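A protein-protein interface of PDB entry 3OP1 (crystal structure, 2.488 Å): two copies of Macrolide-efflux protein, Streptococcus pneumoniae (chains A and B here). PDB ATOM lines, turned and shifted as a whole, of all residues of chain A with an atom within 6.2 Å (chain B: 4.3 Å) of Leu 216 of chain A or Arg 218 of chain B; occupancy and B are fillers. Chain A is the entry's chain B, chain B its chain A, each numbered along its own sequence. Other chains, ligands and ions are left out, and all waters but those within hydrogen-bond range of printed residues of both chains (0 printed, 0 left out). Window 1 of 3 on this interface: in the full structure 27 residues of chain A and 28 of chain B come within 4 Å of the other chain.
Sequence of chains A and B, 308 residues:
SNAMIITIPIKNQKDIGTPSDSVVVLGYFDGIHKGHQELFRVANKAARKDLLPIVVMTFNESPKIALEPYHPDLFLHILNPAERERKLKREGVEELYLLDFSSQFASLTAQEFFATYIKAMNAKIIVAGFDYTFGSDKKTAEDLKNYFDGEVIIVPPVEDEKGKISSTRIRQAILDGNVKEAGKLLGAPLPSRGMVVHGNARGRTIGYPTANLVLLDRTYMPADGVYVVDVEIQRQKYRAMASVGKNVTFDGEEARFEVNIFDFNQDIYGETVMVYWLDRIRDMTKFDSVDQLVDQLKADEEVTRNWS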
ATOM      1  N   ARG A 193      15.367 -14.821  29.938  1.00  0.00           N
ATOM      2  CA  ARG A 193      13.938 -14.851  30.249  1.00  0.00           C
ATOM      3  C   ARG A 193      13.553 -16.019  31.215  1.00  0.00           C
ATOM      4  O   ARG A 193      13.685 -17.203  30.888  1.00  0.00           O
ATOM      5  CB  ARG A 193      13.134 -14.916  28.961  1.00  0.00           C
ATOM      6  CG  ARG A 193      11.645 -14.884  29.167  1.00  0.00           C
ATOM      7  CD  ARG A 193      10.925 -14.863  27.869  1.00  0.00           C
ATOM      8  NE  ARG A 193      11.123 -16.121  27.187  1.00  0.00           N
ATOM      9  CZ  ARG A 193      10.125 -16.906  26.802  1.00  0.00           C
ATOM     10  NH1 ARG A 193       8.870 -16.516  27.016  1.00  0.00           N
ATOM     11  NH2 ARG A 193      10.385 -18.063  26.192  1.00  0.00           N
ATOM     12  N   GLY A 194      13.066 -15.655  32.397  1.00  0.00           N
ATOM     13  CA  GLY A 194      12.739 -16.588  33.456  1.00  0.00           C
ATOM     14  C   GLY A 194      11.267 -16.573  33.811  1.00  0.00           C
ATOM     15  O   GLY A 194      10.557 -15.630  33.472  1.00  0.00           O
ATOM     16  N   MET A 195      10.790 -17.602  34.491  1.00  0.00           N
ATOM     17  CA  MET A 195       9.439 -17.574  35.021  1.00  0.00           C
ATOM     18  C   MET A 195       9.472 -17.828  36.516  1.00  0.00           C
ATOM     19  O   MET A 195      10.112 -18.756  36.966  1.00  0.00           O
ATOM     20  CB  MET A 195       8.511 -18.577  34.346  1.00  0.00           C
ATOM     21  CG  MET A 195       7.127 -18.571  34.968  1.00  0.00           C
ATOM     22  SD  MET A 195       5.702 -19.449  33.994  1.00  0.00           S
ATOM     23  CE  MET A 195       5.621 -18.273  32.485  1.00  0.00           C
ATOM     24  N   VAL A 214      12.640 -20.335  36.738  1.00  0.00           N
ATOM     25  CA  VAL A 214      12.979 -21.334  35.763  1.00  0.00           C
ATOM     26  C   VAL A 214      13.191 -20.626  34.450  1.00  0.00           C
ATOM     27  O   VAL A 214      12.279 -19.944  33.964  1.00  0.00           O
ATOM     28  CB  VAL A 214      11.850 -22.344  35.552  1.00  0.00           C
ATOM     29  CG1 VAL A 214      12.154 -23.242  34.338  1.00  0.00           C
ATOM     30  CG2 VAL A 214      11.648 -23.181  36.781  1.00  0.00           C
ATOM     31  N   LEU A 215      14.397 -20.779  33.897  1.00  0.00           N
ATOM     32  CA  LEU A 215      14.770 -20.277  32.558  1.00  0.00           C
ATOM     33  C   LEU A 215      13.822 -20.836  31.489  1.00  0.00           C
ATOM     34  O   LEU A 215      13.607 -22.045  31.437  1.00  0.00           O
ATOM     35  CB  LEU A 215      16.221 -20.690  32.224  1.00  0.00           C
ATOM     36  CG  LEU A 215      16.914 -20.258  30.929  1.00  0.00           C
ATOM     37  CD1 LEU A 215      16.871 -18.684  30.738  1.00  0.00           C
ATOM     38  CD2 LEU A 215      18.322 -20.811  30.884  1.00  0.00           C
ATOM     39  N   LEU A 216      13.260 -19.982  30.630  1.00  0.00           N
ATOM     40  CA  LEU A 216      12.253 -20.487  29.687  1.00  0.00           C
ATOM     41  C   LEU A 216      12.808 -20.918  28.333  1.00  0.00           C
ATOM     42  O   LEU A 216      12.068 -21.449  27.493  1.00  0.00           O
ATOM     43  CB  LEU A 216      11.141 -19.473  29.483  1.00  0.00           C
ATOM     44  CG  LEU A 216      10.163 -19.390  30.656  1.00  0.00           C
ATOM     45  CD1 LEU A 216       9.241 -18.142  30.525  1.00  0.00           C
ATOM     46  CD2 LEU A 216       9.385 -20.694  30.753  1.00  0.00           C
ATOM     47  N   ASP A 217      14.105 -20.705  28.139  1.00  0.00           N
ATOM     48  CA  ASP A 217      14.711 -20.834  26.837  1.00  0.00           C
ATOM     49  C   ASP A 217      15.997 -21.624  26.906  1.00  0.00           C
ATOM     50  O   ASP A 217      16.617 -21.672  27.951  1.00  0.00           O
ATOM     51  CB  ASP A 217      15.073 -19.436  26.272  1.00  0.00           C
ATOM     52  CG  ASP A 217      13.878 -18.494  26.186  1.00  0.00           C
ATOM     53  OD1 ASP A 217      12.905 -18.815  25.463  1.00  0.00           O
ATOM     54  OD2 ASP A 217      13.925 -17.419  26.834  1.00  0.00           O
ATOM     55  N   ARG A 218      16.429 -22.148  25.757  1.00  0.00           N
ATOM     56  CA  ARG A 218      17.736 -22.778  25.590  1.00  0.00           C
ATOM     57  C   ARG A 218      18.832 -21.744  25.313  1.00  0.00           C
ATOM     58  O   ARG A 218      19.350 -21.628  24.179  1.00  0.00           O
ATOM     59  CB  ARG A 218      17.680 -23.827  24.468  1.00  0.00           C
ATOM     60  CG  ARG A 218      16.565 -24.859  24.614  1.00  0.00           C
ATOM     61  CD  ARG A 218      16.617 -25.816  23.438  1.00  0.00           C
ATOM     62  NE  ARG A 218      15.417 -25.822  22.588  1.00  0.00           N
ATOM     63  CZ  ARG A 218      15.368 -25.288  21.370  1.00  0.00           C
ATOM     64  NH1 ARG A 218      16.448 -24.681  20.848  1.00  0.00           N
ATOM     65  NH2 ARG A 218      14.231 -25.347  20.679  1.00  0.00           N
ATOM     66  N   THR A 272       6.543 -13.866  33.920  1.00  0.00           N
ATOM     67  CA  THR A 272       7.800 -13.993  33.225  1.00  0.00           C
ATOM     68  C   THR A 272       8.608 -12.781  33.677  1.00  0.00           C
ATOM     69  O   THR A 272       8.053 -11.721  33.863  1.00  0.00           O
ATOM     70  CB  THR A 272       7.596 -13.909  31.697  1.00  0.00           C
ATOM     71  OG1 THR A 272       6.789 -14.996  31.233  1.00  0.00           O
ATOM     72  CG2 THR A 272       8.929 -13.912  30.948  1.00  0.00           C
ATOM     73  N   GLU B  61       1.375 -20.794  30.109  1.00  0.00           N
ATOM     74  CA  GLU B  61       1.749 -21.958  30.885  1.00  0.00           C
ATOM     75  C   GLU B  61       0.611 -22.339  31.809  1.00  0.00           C
ATOM     76  O   GLU B  61      -0.240 -21.521  32.115  1.00  0.00           O
ATOM     77  CB  GLU B  61       3.046 -21.673  31.667  1.00  0.00           C
ATOM     78  CG  GLU B  61       4.204 -21.255  30.772  1.00  0.00           C
ATOM     79  CD  GLU B  61       4.703 -22.363  29.776  1.00  0.00           C
ATOM     80  OE1 GLU B  61       4.320 -23.550  29.890  1.00  0.00           O
ATOM     81  OE2 GLU B  61       5.523 -22.050  28.889  1.00  0.00           O
ATOM     82  N   PHE B  75       5.335 -27.730  33.213  1.00  0.00           N
ATOM     83  CA  PHE B  75       5.645 -27.112  31.926  1.00  0.00           C
ATOM     84  C   PHE B  75       5.265 -27.926  30.700  1.00  0.00           C
ATOM     85  O   PHE B  75       5.659 -27.581  29.610  1.00  0.00           O
ATOM     86  CB  PHE B  75       7.140 -26.787  31.858  1.00  0.00           C
ATOM     87  CG  PHE B  75       7.492 -25.495  32.573  1.00  0.00           C
ATOM     88  CD1 PHE B  75       7.210 -24.263  31.987  1.00  0.00           C
ATOM     89  CD2 PHE B  75       8.012 -25.511  33.842  1.00  0.00           C
ATOM     90  CE1 PHE B  75       7.484 -23.109  32.641  1.00  0.00           C
ATOM     91  CE2 PHE B  75       8.292 -24.326  34.509  1.00  0.00           C
ATOM     92  CZ  PHE B  75       8.031 -23.135  33.904  1.00  0.00           C
ATOM     93  N   LEU B  76       4.521 -29.012  30.848  1.00  0.00           N
ATOM     94  CA  LEU B  76       4.324 -29.827  29.686  1.00  0.00           C
ATOM     95  C   LEU B  76       3.015 -29.468  29.027  1.00  0.00           C
ATOM     96  O   LEU B  76       1.982 -29.399  29.687  1.00  0.00           O
ATOM     97  CB  LEU B  76       4.359 -31.316  30.049  1.00  0.00           C
ATOM     98  CG  LEU B  76       5.742 -31.853  30.361  1.00  0.00           C
ATOM     99  CD1 LEU B  76       5.600 -33.253  30.918  1.00  0.00           C
ATOM    100  CD2 LEU B  76       6.580 -31.840  29.098  1.00  0.00           C
ATOM    101  N   HIS B  77       3.036 -29.322  27.712  1.00  0.00           N
ATOM    102  CA  HIS B  77       1.847 -28.985  26.950  1.00  0.00           C
ATOM    103  C   HIS B  77       1.460 -30.138  26.050  1.00  0.00           C
ATOM    104  O   HIS B  77       2.323 -30.849  25.575  1.00  0.00           O
ATOM    105  CB  HIS B  77       2.126 -27.784  26.053  1.00  0.00           C
ATOM    106  CG  HIS B  77       2.218 -26.484  26.779  1.00  0.00           C
ATOM    107  ND1 HIS B  77       1.117 -25.710  27.056  1.00  0.00           N
ATOM    108  CD2 HIS B  77       3.283 -25.810  27.269  1.00  0.00           C
ATOM    109  CE1 HIS B  77       1.496 -24.622  27.696  1.00  0.00           C
ATOM    110  NE2 HIS B  77       2.806 -24.659  27.837  1.00  0.00           N
ATOM    111  N   ASP B 217       9.868 -29.293  21.703  1.00  0.00           N
ATOM    112  CA  ASP B 217       8.926 -28.580  22.542  1.00  0.00           C
ATOM    113  C   ASP B 217       8.657 -29.317  23.824  1.00  0.00           C
ATOM    114  O   ASP B 217       8.882 -30.511  23.922  1.00  0.00           O
ATOM    115  CB  ASP B 217       7.599 -28.356  21.822  1.00  0.00           C
ATOM    116  CG  ASP B 217       7.775 -27.878  20.421  1.00  0.00           C
ATOM    117  OD1 ASP B 217       8.056 -26.687  20.226  1.00  0.00           O
ATOM    118  OD2 ASP B 217       7.629 -28.694  19.506  1.00  0.00           O
ATOM    119  N   ARG B 218       8.170 -28.580  24.807  1.00  0.00           N
ATOM    120  CA  ARG B 218       7.785 -29.162  26.066  1.00  0.00           C
ATOM    121  C   ARG B 218       6.384 -29.706  25.877  1.00  0.00           C
ATOM    122  O   ARG B 218       5.412 -29.168  26.379  1.00  0.00           O
ATOM    123  CB  ARG B 218       7.789 -28.111  27.159  1.00  0.00           C
ATOM    124  CG  ARG B 218       9.101 -27.398  27.335  1.00  0.00           C
ATOM    125  CD  ARG B 218       9.010 -26.399  28.460  1.00  0.00           C
ATOM    126  NE  ARG B 218       9.209 -25.030  28.013  1.00  0.00           N
ATOM    127  CZ  ARG B 218       8.282 -24.085  28.060  1.00  0.00           C
ATOM    128  NH1 ARG B 218       7.080 -24.356  28.530  1.00  0.00           N
ATOM    129  NH2 ARG B 218       8.558 -22.869  27.633  1.00  0.00           N
ATOM    130  N   THR B 219       6.308 -30.798  25.141  1.00  0.00           N
ATOM    131  CA  THR B 219       5.053 -31.435  24.850  1.00  0.00           C
ATOM    132  C   THR B 219       5.170 -32.855  25.307  1.00  0.00           C
ATOM    133  O   THR B 219       6.253 -33.402  25.389  1.00  0.00           O
ATOM    134  CB  THR B 219       4.718 -31.415  23.357  1.00  0.00           C
ATOM    135  OG1 THR B 219       5.902 -31.637  22.597  1.00  0.00           O
ATOM    136  CG2 THR B 219       4.111 -30.095  22.970  1.00  0.00           C
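A ring nitrogen (NE2) of His 77 of chain B sits at hydrogen-bond distance from the side-chain carboxylate of Glu 61 of chain B (2.8 Å).
The guanidinium group (NH1) of Arg 218 of chain B lies within salt-bridge range of the side-chain carboxylate (OE2) of Glu 61 of chain B (2.8 Å).
The backbone NH (N) of His 77 of chain B lies within hydrogen-bond range of the backbone carbonyl oxygen (O) of Arg 218 of chain B, 2.7 Å away.
The backbone carbonyl oxygen (O) of Arg 193 of chain A is in hydrogen-bond range of the backbone NH (N) of Leu 216 of chain A, at 2.8 Å.
The backbone NH (N) of Met 195 of chain A is in hydrogen-bond range of the backbone carbonyl oxygen (O) of Val 214 of chain A, at 2.8 Å.
Hydrophobic or aromatic side chains of chain A within 4 Å of the printed part of chain B: Met 195 and Leu 216.
Of the 7 printed residues of chain B, 3 touch a printed residue of chain A.
Among the printed residues, 3 pairs touch across the chains.
Of the printed residues of chain B, Met 195 of chain A touches Glu 61 (3.7 Å).
Leu 216 of chain A touches two residues of chain B.
Asp 217 of chain A touches none of the printed residues of chain B.
Thr 272 of chain A touches none of the printed residues of chain B.
Printed residues of chain A within 4 Å of Glu 61 of chain B: Met 195.
Of the printed residues of chain A, Phe 75 of chain B touches Leu 216 (3.6 Å).
Arg 218 of chain B touches one residue of chain A.
The nearest printed residue of chain A that does not touch Phe 75 of chain B is Val 214 of chain A (4.01 Å).
Positions printed for both chains: 217 and 218.
Of the 3 pairs that touch across the chains among the printed residues, none has its exchanged pair printed and touching as well.
Glu 61 of chain B touches Met 195 of chain A (CG to CE, 3.7 Å).
Leu 216 of chain A touches Phe 75 of chain B.
Arg 218 of chain B touches Leu 216 of chain A (NH2 to O, 3.8 Å).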
